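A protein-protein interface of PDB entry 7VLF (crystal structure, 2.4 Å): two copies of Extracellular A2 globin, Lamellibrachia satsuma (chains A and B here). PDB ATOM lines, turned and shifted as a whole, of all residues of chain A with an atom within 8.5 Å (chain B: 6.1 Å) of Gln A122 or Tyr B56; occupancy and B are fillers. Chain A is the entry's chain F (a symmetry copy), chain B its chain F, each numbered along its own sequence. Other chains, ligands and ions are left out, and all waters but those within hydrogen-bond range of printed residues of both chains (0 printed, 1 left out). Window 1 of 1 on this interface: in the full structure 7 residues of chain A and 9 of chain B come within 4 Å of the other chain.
The guanidinium group of Arg B61 lies within salt-bridge range of the side-chain carboxylate of Glu B26 (3.5 Å). The side-chain amide oxygen of Asn B54 lies within hydrogen-bond range of the backbone NH of Tyr B56, 2.9 Å away. The backbone carbonyl oxygen (O) of Asn B54 lies within hydrogen-bond range of the side-chain hydroxyl (OG1) of Thr B57 (2.5 Å). The guanidinium group (NE) of Arg B61 is in hydrogen-bond range of the backbone carbonyl oxygen (O) of Tyr B56, 3.4 Å away. The side-chain carboxylate (OD1) of Asp A126 is in hydrogen-bond range of the backbone NH (N) of Asp A128 (3.2 Å).
Printed residues of chain A that touch a printed residue of chain B: Met A114, Glu A117, Gln A122, Asn A123, Phe A125, Lys A127 and Asp A128. Hydrophobic or aromatic side chains of chain A within 4 Å of the printed part of chain B: Met A114 and Phe A125. Printed residues of chain B that touch a printed residue of chain A: Glu B26, Glu B27, His B30, Asn B54, Tyr B56, Thr B57 and Arg B61.
OE1 of Glu B26 sits at hydrogen-bond distance from NE2 of Gln A122, at 3.4 Å. ND2 of Asn B54 lies close to N of Asp A128, 3.1 Å away. The side-chain amide oxygen of Gln A122 sits at hydrogen-bond distance from the guanidinium group of Arg B61 (3.0 Å).
Tyr B56 touches Met A114. NE2 of His B30 touches OE2 of Glu A117, 3.8 Å away. Glu A117 touches Tyr B56. NE2 of Gln A122 touches CA of Glu B27, at 3.9 Å. Asn A123 touches Glu B26. Asn A123 touches Arg B61. Tyr B56 touches Phe A125 (CZ to CD2, 3.5 Å). CB of Lys A127 touches OD1 of Asn B54 (3.4 Å). Lys A127 touches Tyr B56. CG2 of Thr B57 touches OD2 of Asp A128 (3.8 Å).
Of chain B, only Glu B26 (3.4 Å), Glu B27 (3.9 Å), His B30 (3.8 Å), Tyr B56 (3.2 Å) and Arg B61 (2.3 Å) come within 4 Å of Gln A122. Tyr B56 touches just these residues of chain A: Met A114, Glu A117, Gln A122, Phe A125 and Lys A127. Of chain A, only Asp A128 comes within 4 Å of Thr B57. Of the printed residues of chain B, Met A114 touches Tyr B56 (3.9 Å). Of the printed residues of chain A, Arg B61 touches Gln A122 (2.3 Å) and Asn A123 (3.8 Å). Of the printed residues of chain A, His B30 touches Glu A117 (3.8 Å) and Gln A122 (3.8 Å). The nearest residue of chain A that does not touch Tyr B56 is Met A113 (5.0 Å).
No position is printed for both chains. Of the 15 pairs that touch across the chains among the printed residues, none has its exchanged pair printed and touching as well.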
ATOM      1  N   GLN A  14       6.498 -18.894 -19.035  1.00  0.00           N
ATOM      2  CA  GLN A  14       7.306 -17.681 -19.107  1.00  0.00           C
ATOM      3  C   GLN A  14       6.534 -16.506 -19.692  1.00  0.00           C
ATOM      4  O   GLN A  14       6.908 -15.355 -19.445  1.00  0.00           O
ATOM      5  CB  GLN A  14       8.577 -17.937 -19.919  1.00  0.00           C
ATOM      6  CG  GLN A  14       9.466 -19.008 -19.313  1.00  0.00           C
ATOM      7  CD  GLN A  14      10.913 -18.883 -19.734  1.00  0.00           C
ATOM      8  OE1 GLN A  14      11.224 -18.779 -20.918  1.00  0.00           O
ATOM      9  NE2 GLN A  14      11.813 -18.886 -18.756  1.00  0.00           N
ATOM     10  N   HIS A 110      11.167 -10.565 -32.419  1.00  0.00           N
ATOM     11  CA  HIS A 110      12.344 -10.206 -31.640  1.00  0.00           C
ATOM     12  C   HIS A 110      12.008  -9.205 -30.545  1.00  0.00           C
ATOM     13  O   HIS A 110      12.644  -9.208 -29.485  1.00  0.00           O
ATOM     14  CB  HIS A 110      13.422  -9.646 -32.566  1.00  0.00           C
ATOM     15  CG  HIS A 110      14.661  -9.206 -31.853  1.00  0.00           C
ATOM     16  ND1 HIS A 110      14.863  -7.905 -31.444  1.00  0.00           N
ATOM     17  CD2 HIS A 110      15.765  -9.894 -31.476  1.00  0.00           C
ATOM     18  CE1 HIS A 110      16.036  -7.812 -30.846  1.00  0.00           C
ATOM     19  NE2 HIS A 110      16.605  -9.005 -30.852  1.00  0.00           N
ATOM     20  N   MET A 113      10.554 -11.187 -27.706  1.00  0.00           N
ATOM     21  CA  MET A 113      11.616 -11.929 -27.035  1.00  0.00           C
ATOM     22  C   MET A 113      12.476 -11.021 -26.167  1.00  0.00           C
ATOM     23  O   MET A 113      13.091 -11.488 -25.202  1.00  0.00           O
ATOM     24  CB  MET A 113      12.480 -12.656 -28.065  1.00  0.00           C
ATOM     25  CG  MET A 113      11.788 -13.838 -28.720  1.00  0.00           C
ATOM     26  SD  MET A 113      12.870 -14.838 -29.762  1.00  0.00           S
ATOM     27  CE  MET A 113      13.188 -13.713 -31.119  1.00  0.00           C
ATOM     28  N   MET A 114      12.540  -9.729 -26.492  1.00  0.00           N
ATOM     29  CA  MET A 114      13.256  -8.794 -25.634  1.00  0.00           C
ATOM     30  C   MET A 114      12.422  -8.404 -24.419  1.00  0.00           C
ATOM     31  O   MET A 114      12.952  -8.300 -23.308  1.00  0.00           O
ATOM     32  CB  MET A 114      13.659  -7.551 -26.429  1.00  0.00           C
ATOM     33  CG  MET A 114      14.668  -7.807 -27.544  1.00  0.00           C
ATOM     34  SD  MET A 114      16.214  -8.561 -26.990  1.00  0.00           S
ATOM     35  CE  MET A 114      15.943 -10.285 -27.407  1.00  0.00           C
ATOM     36  N   GLY A 115      11.120  -8.186 -24.612  1.00  0.00           N
ATOM     37  CA  GLY A 115      10.268  -7.839 -23.489  1.00  0.00           C
ATOM     38  C   GLY A 115      10.072  -8.995 -22.528  1.00  0.00           C
ATOM     39  O   GLY A 115      10.127  -8.814 -21.308  1.00  0.00           O
ATOM     40  N   VAL A 116       9.832 -10.194 -23.061  1.00  0.00           N
ATOM     41  CA  VAL A 116       9.669 -11.369 -22.211  1.00  0.00           C
ATOM     42  C   VAL A 116      10.938 -11.615 -21.406  1.00  0.00           C
ATOM     43  O   VAL A 116      10.890 -11.848 -20.192  1.00  0.00           O
ATOM     44  CB  VAL A 116       9.286 -12.595 -23.060  1.00  0.00           C
ATOM     45  CG1 VAL A 116       9.386 -13.863 -22.234  1.00  0.00           C
ATOM     46  CG2 VAL A 116       7.879 -12.429 -23.613  1.00  0.00           C
ATOM     47  N   GLU A 117      12.096 -11.551 -22.067  1.00  0.00           N
ATOM     48  CA  GLU A 117      13.361 -11.671 -21.349  1.00  0.00           C
ATOM     49  C   GLU A 117      13.522 -10.542 -20.340  1.00  0.00           C
ATOM     50  O   GLU A 117      14.061 -10.747 -19.245  1.00  0.00           O
ATOM     51  CB  GLU A 117      14.526 -11.680 -22.339  1.00  0.00           C
ATOM     52  CG  GLU A 117      15.893 -11.900 -21.708  1.00  0.00           C
ATOM     53  CD  GLU A 117      16.666 -10.612 -21.512  1.00  0.00           C
ATOM     54  OE1 GLU A 117      16.037  -9.537 -21.422  1.00  0.00           O
ATOM     55  OE2 GLU A 117      17.913 -10.677 -21.456  1.00  0.00           O
ATOM     56  N   HIS A 118      13.066  -9.339 -20.696  1.00  0.00           N
ATOM     57  CA  HIS A 118      13.163  -8.200 -19.790  1.00  0.00           C
ATOM     58  C   HIS A 118      12.374  -8.429 -18.507  1.00  0.00           C
ATOM     59  O   HIS A 118      12.776  -7.955 -17.439  1.00  0.00           O
ATOM     60  CB  HIS A 118      12.674  -6.936 -20.499  1.00  0.00           C
ATOM     61  CG  HIS A 118      12.466  -5.771 -19.584  1.00  0.00           C
ATOM     62  ND1 HIS A 118      13.502  -5.142 -18.929  1.00  0.00           N
ATOM     63  CD2 HIS A 118      11.337  -5.115 -19.220  1.00  0.00           C
ATOM     64  CE1 HIS A 118      13.021  -4.151 -18.198  1.00  0.00           C
ATOM     65  NE2 HIS A 118      11.710  -4.115 -18.357  1.00  0.00           N
ATOM     66  N   GLU A 119      11.261  -9.159 -18.587  1.00  0.00           N
ATOM     67  CA  GLU A 119      10.432  -9.368 -17.407  1.00  0.00           C
ATOM     68  C   GLU A 119      10.938 -10.524 -16.552  1.00  0.00           C
ATOM     69  O   GLU A 119      10.891 -10.451 -15.319  1.00  0.00           O
ATOM     70  CB  GLU A 119       8.984  -9.615 -17.823  1.00  0.00           C
ATOM     71  CG  GLU A 119       8.374  -8.499 -18.655  1.00  0.00           C
ATOM     72  CD  GLU A 119       8.299  -7.185 -17.906  1.00  0.00           C
ATOM     73  OE1 GLU A 119       8.024  -7.207 -16.687  1.00  0.00           O
ATOM     74  OE2 GLU A 119       8.518  -6.132 -18.540  1.00  0.00           O
ATOM     75  N   ILE A 120      11.420 -11.596 -17.178  1.00  0.00           N
ATOM     76  CA  ILE A 120      11.771 -12.805 -16.441  1.00  0.00           C
ATOM     77  C   ILE A 120      13.266 -12.943 -16.170  1.00  0.00           C
ATOM     78  O   ILE A 120      13.644 -13.617 -15.200  1.00  0.00           O
ATOM     79  CB  ILE A 120      11.249 -14.062 -17.168  1.00  0.00           C
ATOM     80  CG1 ILE A 120      11.994 -14.267 -18.487  1.00  0.00           C
ATOM     81  CG2 ILE A 120       9.750 -13.953 -17.408  1.00  0.00           C
ATOM     82  CD1 ILE A 120      11.509 -15.451 -19.281  1.00  0.00           C
ATOM     83  N   GLY A 121      14.115 -12.335 -16.976  1.00  0.00           N
ATOM     84  CA  GLY A 121      15.537 -12.442 -16.729  1.00  0.00           C
ATOM     85  C   GLY A 121      16.235 -13.231 -17.823  1.00  0.00           C
ATOM     86  O   GLY A 121      15.650 -14.116 -18.463  1.00  0.00           O
ATOM     87  N   GLN A 122      17.511 -12.911 -18.038  1.00  0.00           N
ATOM     88  CA  GLN A 122      18.234 -13.514 -19.152  1.00  0.00           C
ATOM     89  C   GLN A 122      18.620 -14.957 -18.863  1.00  0.00           C
ATOM     90  O   GLN A 122      18.704 -15.773 -19.790  1.00  0.00           O
ATOM     91  CB  GLN A 122      19.476 -12.686 -19.486  1.00  0.00           C
ATOM     92  CG  GLN A 122      20.480 -12.537 -18.355  1.00  0.00           C
ATOM     93  CD  GLN A 122      21.509 -13.649 -18.328  1.00  0.00           C
ATOM     94  OE1 GLN A 122      21.627 -14.427 -19.275  1.00  0.00           O
ATOM     95  NE2 GLN A 122      22.259 -13.733 -17.236  1.00  0.00           N
ATOM     96  N   ASN A 123      18.872 -15.293 -17.596  1.00  0.00           N
ATOM     97  CA  ASN A 123      19.319 -16.641 -17.272  1.00  0.00           C
ATOM     98  C   ASN A 123      18.211 -17.666 -17.473  1.00  0.00           C
ATOM     99  O   ASN A 123      18.489 -18.813 -17.843  1.00  0.00           O
ATOM    100  CB  ASN A 123      19.835 -16.682 -15.837  1.00  0.00           C
ATOM    101  CG  ASN A 123      18.782 -16.266 -14.833  1.00  0.00           C
ATOM    102  OD1 ASN A 123      17.849 -15.530 -15.160  1.00  0.00           O
ATOM    103  ND2 ASN A 123      18.924 -16.739 -13.601  1.00  0.00           N
ATOM    104  N   VAL A 124      16.956 -17.273 -17.254  1.00  0.00           N
ATOM    105  CA  VAL A 124      15.840 -18.201 -17.389  1.00  0.00           C
ATOM    106  C   VAL A 124      15.195 -18.157 -18.770  1.00  0.00           C
ATOM    107  O   VAL A 124      14.470 -19.094 -19.134  1.00  0.00           O
ATOM    108  CB  VAL A 124      14.777 -17.922 -16.312  1.00  0.00           C
ATOM    109  CG1 VAL A 124      15.405 -17.982 -14.928  1.00  0.00           C
ATOM    110  CG2 VAL A 124      14.122 -16.573 -16.549  1.00  0.00           C
ATOM    111  N   PHE A 125      15.441 -17.106 -19.547  1.00  0.00           N
ATOM    112  CA  PHE A 125      14.809 -16.971 -20.852  1.00  0.00           C
ATOM    113  C   PHE A 125      15.389 -17.978 -21.838  1.00  0.00           C
ATOM    114  O   PHE A 125      16.610 -18.101 -21.975  1.00  0.00           O
ATOM    115  CB  PHE A 125      14.988 -15.546 -21.373  1.00  0.00           C
ATOM    116  CG  PHE A 125      14.472 -15.338 -22.766  1.00  0.00           C
ATOM    117  CD1 PHE A 125      13.114 -15.200 -23.005  1.00  0.00           C
ATOM    118  CD2 PHE A 125      15.346 -15.272 -23.839  1.00  0.00           C
ATOM    119  CE1 PHE A 125      12.637 -15.007 -24.289  1.00  0.00           C
ATOM    120  CE2 PHE A 125      14.874 -15.078 -25.124  1.00  0.00           C
ATOM    121  CZ  PHE A 125      13.518 -14.945 -25.349  1.00  0.00           C
ATOM    122  N   ASP A 126      14.506 -18.699 -22.524  1.00  0.00           N
ATOM    123  CA  ASP A 126      14.882 -19.678 -23.538  1.00  0.00           C
ATOM    124  C   ASP A 126      14.584 -19.079 -24.905  1.00  0.00           C
ATOM    125  O   ASP A 126      13.420 -18.969 -25.298  1.00  0.00           O
ATOM    126  CB  ASP A 126      14.129 -20.991 -23.332  1.00  0.00           C
ATOM    127  CG  ASP A 126      14.706 -22.135 -24.151  1.00  0.00           C
ATOM    128  OD1 ASP A 126      15.427 -21.875 -25.135  1.00  0.00           O
ATOM    129  OD2 ASP A 126      14.433 -23.305 -23.807  1.00  0.00           O
ATOM    130  N   LYS A 127      15.637 -18.705 -25.634  1.00  0.00           N
ATOM    131  CA  LYS A 127      15.441 -18.107 -26.951  1.00  0.00           C
ATOM    132  C   LYS A 127      15.023 -19.150 -27.980  1.00  0.00           C
ATOM    133  O   LYS A 127      14.176 -18.875 -28.838  1.00  0.00           O
ATOM    134  CB  LYS A 127      16.717 -17.392 -27.394  1.00  0.00           C
ATOM    135  CG  LYS A 127      16.654 -16.812 -28.796  1.00  0.00           C
ATOM    136  CD  LYS A 127      17.900 -15.998 -29.109  1.00  0.00           C
ATOM    137  CE  LYS A 127      17.907 -15.529 -30.555  1.00  0.00           C
ATOM    138  NZ  LYS A 127      17.972 -16.676 -31.500  1.00  0.00           N
ATOM    139  N   ASP A 128      15.602 -20.352 -27.912  1.00  0.00           N
ATOM    140  CA  ASP A 128      15.277 -21.384 -28.894  1.00  0.00           C
ATOM    141  C   ASP A 128      13.802 -21.757 -28.842  1.00  0.00           C
ATOM    142  O   ASP A 128      13.157 -21.911 -29.887  1.00  0.00           O
ATOM    143  CB  ASP A 128      16.145 -22.624 -28.672  1.00  0.00           C
ATOM    144  CG  ASP A 128      17.453 -22.564 -29.432  1.00  0.00           C
ATOM    145  OD1 ASP A 128      17.494 -21.930 -30.506  1.00  0.00           O
ATOM    146  OD2 ASP A 128      18.443 -23.157 -28.956  1.00  0.00           O
ATOM    147  N   TRP A 130      11.289 -19.917 -27.664  1.00  0.00           N
ATOM    148  CA  TRP A 130      10.430 -18.793 -28.021  1.00  0.00           C
ATOM    149  C   TRP A 130      10.505 -18.488 -29.513  1.00  0.00           C
ATOM    150  O   TRP A 130       9.473 -18.309 -30.169  1.00  0.00           O
ATOM    151  CB  TRP A 130      10.807 -17.565 -27.195  1.00  0.00           C
ATOM    152  CG  TRP A 130      10.153 -17.529 -25.846  1.00  0.00           C
ATOM    153  CD1 TRP A 130      10.628 -18.074 -24.688  1.00  0.00           C
ATOM    154  CD2 TRP A 130       8.903 -16.915 -25.516  1.00  0.00           C
ATOM    155  NE1 TRP A 130       9.751 -17.836 -23.659  1.00  0.00           N
ATOM    156  CE2 TRP A 130       8.684 -17.127 -24.140  1.00  0.00           C
ATOM    157  CE3 TRP A 130       7.946 -16.207 -26.250  1.00  0.00           C
ATOM    158  CZ2 TRP A 130       7.549 -16.656 -23.484  1.00  0.00           C
ATOM    159  CZ3 TRP A 130       6.821 -15.740 -25.597  1.00  0.00           C
ATOM    160  CH2 TRP A 130       6.632 -15.966 -24.228  1.00  0.00           C
ATOM    161  N   GLU B  26      28.014 -14.287 -15.349  1.00  0.00           N
ATOM    162  CA  GLU B  26      27.105 -14.693 -16.414  1.00  0.00           C
ATOM    163  C   GLU B  26      26.345 -13.496 -16.968  1.00  0.00           C
ATOM    164  O   GLU B  26      26.149 -13.381 -18.183  1.00  0.00           O
ATOM    165  CB  GLU B  26      26.131 -15.752 -15.898  1.00  0.00           C
ATOM    166  CG  GLU B  26      25.378 -16.493 -16.989  1.00  0.00           C
ATOM    167  CD  GLU B  26      24.165 -17.233 -16.460  1.00  0.00           C
ATOM    168  OE1 GLU B  26      23.357 -16.607 -15.741  1.00  0.00           O
ATOM    169  OE2 GLU B  26      24.021 -18.438 -16.754  1.00  0.00           O
ATOM    170  N   GLU B  27      25.913 -12.592 -16.088  1.00  0.00           N
ATOM    171  CA  GLU B  27      25.259 -11.370 -16.541  1.00  0.00           C
ATOM    172  C   GLU B  27      26.247 -10.423 -17.210  1.00  0.00           C
ATOM    173  O   GLU B  27      25.877  -9.706 -18.147  1.00  0.00           O
ATOM    174  CB  GLU B  27      24.568 -10.689 -15.357  1.00  0.00           C
ATOM    175  CG  GLU B  27      23.853  -9.386 -15.684  1.00  0.00           C
ATOM    176  CD  GLU B  27      24.768  -8.178 -15.604  1.00  0.00           C
ATOM    177  OE1 GLU B  27      24.492  -7.172 -16.292  1.00  0.00           O
ATOM    178  OE2 GLU B  27      25.767  -8.240 -14.858  1.00  0.00           O
ATOM    179  N   HIS B  30      27.134 -11.812 -20.843  1.00  0.00           N
ATOM    180  CA  HIS B  30      25.940 -11.716 -21.674  1.00  0.00           C
ATOM    181  C   HIS B  30      25.682 -10.277 -22.103  1.00  0.00           C
ATOM    182  O   HIS B  30      25.250 -10.026 -23.233  1.00  0.00           O
ATOM    183  CB  HIS B  30      24.733 -12.276 -20.924  1.00  0.00           C
ATOM    184  CG  HIS B  30      23.431 -12.040 -21.620  1.00  0.00           C
ATOM    185  ND1 HIS B  30      22.960 -12.863 -22.620  1.00  0.00           N
ATOM    186  CD2 HIS B  30      22.503 -11.066 -21.466  1.00  0.00           C
ATOM    187  CE1 HIS B  30      21.796 -12.409 -23.049  1.00  0.00           C
ATOM    188  NE2 HIS B  30      21.495 -11.320 -22.365  1.00  0.00           N
ATOM    189  N   ASN B  54      21.955 -18.269 -30.507  1.00  0.00           N
ATOM    190  CA  ASN B  54      21.302 -18.216 -29.202  1.00  0.00           C
ATOM    191  C   ASN B  54      22.355 -17.903 -28.146  1.00  0.00           C
ATOM    192  O   ASN B  54      23.171 -18.765 -27.800  1.00  0.00           O
ATOM    193  CB  ASN B  54      20.587 -19.529 -28.896  1.00  0.00           C
ATOM    194  CG  ASN B  54      19.662 -19.423 -27.694  1.00  0.00           C
ATOM    195  OD1 ASN B  54      19.844 -18.571 -26.826  1.00  0.00           O
ATOM    196  ND2 ASN B  54      18.664 -20.296 -27.639  1.00  0.00           N
ATOM    197  N   ILE B  55      22.324 -16.672 -27.630  1.00  0.00           N
ATOM    198  CA  ILE B  55      23.281 -16.257 -26.608  1.00  0.00           C
ATOM    199  C   ILE B  55      22.982 -16.942 -25.281  1.00  0.00           C
ATOM    200  O   ILE B  55      23.892 -17.193 -24.480  1.00  0.00           O
ATOM    201  CB  ILE B  55      23.275 -14.722 -26.466  1.00  0.00           C
ATOM    202  CG1 ILE B  55      23.540 -14.050 -27.817  1.00  0.00           C
ATOM    203  CG2 ILE B  55      24.309 -14.269 -25.449  1.00  0.00           C
ATOM    204  CD1 ILE B  55      22.289 -13.631 -28.556  1.00  0.00           C
ATOM    205  N   TYR B  56      21.717 -17.283 -25.036  1.00  0.00           N
ATOM    206  CA  TYR B  56      21.292 -17.870 -23.774  1.00  0.00           C
ATOM    207  C   TYR B  56      21.636 -19.350 -23.648  1.00  0.00           C
ATOM    208  O   TYR B  56      21.426 -19.922 -22.573  1.00  0.00           O
ATOM    209  CB  TYR B  56      19.782 -17.678 -23.594  1.00  0.00           C
ATOM    210  CG  TYR B  56      19.290 -16.282 -23.924  1.00  0.00           C
ATOM    211  CD1 TYR B  56      18.979 -15.927 -25.229  1.00  0.00           C
ATOM    212  CD2 TYR B  56      19.133 -15.323 -22.931  1.00  0.00           C
ATOM    213  CE1 TYR B  56      18.532 -14.659 -25.541  1.00  0.00           C
ATOM    214  CE2 TYR B  56      18.683 -14.048 -23.235  1.00  0.00           C
ATOM    215  CZ  TYR B  56      18.385 -13.724 -24.543  1.00  0.00           C
ATOM    216  OH  TYR B  56      17.937 -12.461 -24.860  1.00  0.00           O
ATOM    217  N   THR B  57      22.148 -19.981 -24.700  1.00  0.00           N
ATOM    218  CA  THR B  57      22.480 -21.399 -24.617  1.00  0.00           C
ATOM    219  C   THR B  57      23.742 -21.601 -23.779  1.00  0.00           C
ATOM    220  O   THR B  57      24.664 -20.779 -23.841  1.00  0.00           O
ATOM    221  CB  THR B  57      22.685 -21.990 -26.011  1.00  0.00           C
ATOM    222  OG1 THR B  57      23.432 -21.072 -26.817  1.00  0.00           O
ATOM    223  CG2 THR B  57      21.344 -22.281 -26.672  1.00  0.00           C
ATOM    224  N   PRO B  58      23.817 -22.679 -22.991  1.00  0.00           N
ATOM    225  CA  PRO B  58      25.033 -22.911 -22.196  1.00  0.00           C
ATOM    226  C   PRO B  58      26.279 -23.092 -23.042  1.00  0.00           C
ATOM    227  O   PRO B  58      27.385 -22.804 -22.566  1.00  0.00           O
ATOM    228  CB  PRO B  58      24.697 -24.183 -21.404  1.00  0.00           C
ATOM    229  CG  PRO B  58      23.215 -24.260 -21.398  1.00  0.00           C
ATOM    230  CD  PRO B  58      22.778 -23.680 -22.714  1.00  0.00           C
ATOM    231  N   PHE B  60      27.140 -21.331 -25.618  1.00  0.00           N
ATOM    232  CA  PHE B  60      27.699 -20.016 -25.908  1.00  0.00           C
ATOM    233  C   PHE B  60      28.241 -19.346 -24.653  1.00  0.00           C
ATOM    234  O   PHE B  60      29.254 -18.640 -24.715  1.00  0.00           O
ATOM    235  CB  PHE B  60      26.653 -19.123 -26.573  1.00  0.00           C
ATOM    236  CG  PHE B  60      27.205 -17.813 -27.058  1.00  0.00           C
ATOM    237  CD1 PHE B  60      28.123 -17.775 -28.092  1.00  0.00           C
ATOM    238  CD2 PHE B  60      26.812 -16.623 -26.475  1.00  0.00           C
ATOM    239  CE1 PHE B  60      28.638 -16.575 -28.540  1.00  0.00           C
ATOM    240  CE2 PHE B  60      27.322 -15.417 -26.920  1.00  0.00           C
ATOM    241  CZ  PHE B  60      28.236 -15.394 -27.954  1.00  0.00           C
ATOM    242  N   ARG B  61      27.585 -19.553 -23.506  1.00  0.00           N
ATOM    243  CA  ARG B  61      28.063 -18.946 -22.268  1.00  0.00           C
ATOM    244  C   ARG B  61      29.435 -19.478 -21.880  1.00  0.00           C
ATOM    245  O   ARG B  61      30.246 -18.739 -21.310  1.00  0.00           O
ATOM    246  CB  ARG B  61      27.061 -19.186 -21.141  1.00  0.00           C
ATOM    247  CG  ARG B  61      25.620 -18.886 -21.511  1.00  0.00           C
ATOM    248  CD  ARG B  61      24.906 -18.149 -20.396  1.00  0.00           C
ATOM    249  NE  ARG B  61      23.470 -18.072 -20.645  1.00  0.00           N
ATOM    250  CZ  ARG B  61      22.671 -17.142 -20.133  1.00  0.00           C
ATOM    251  NH1 ARG B  61      21.375 -17.149 -20.411  1.00  0.00           N
ATOM    252  NH2 ARG B  61      23.169 -16.195 -19.353  1.00  0.00           N
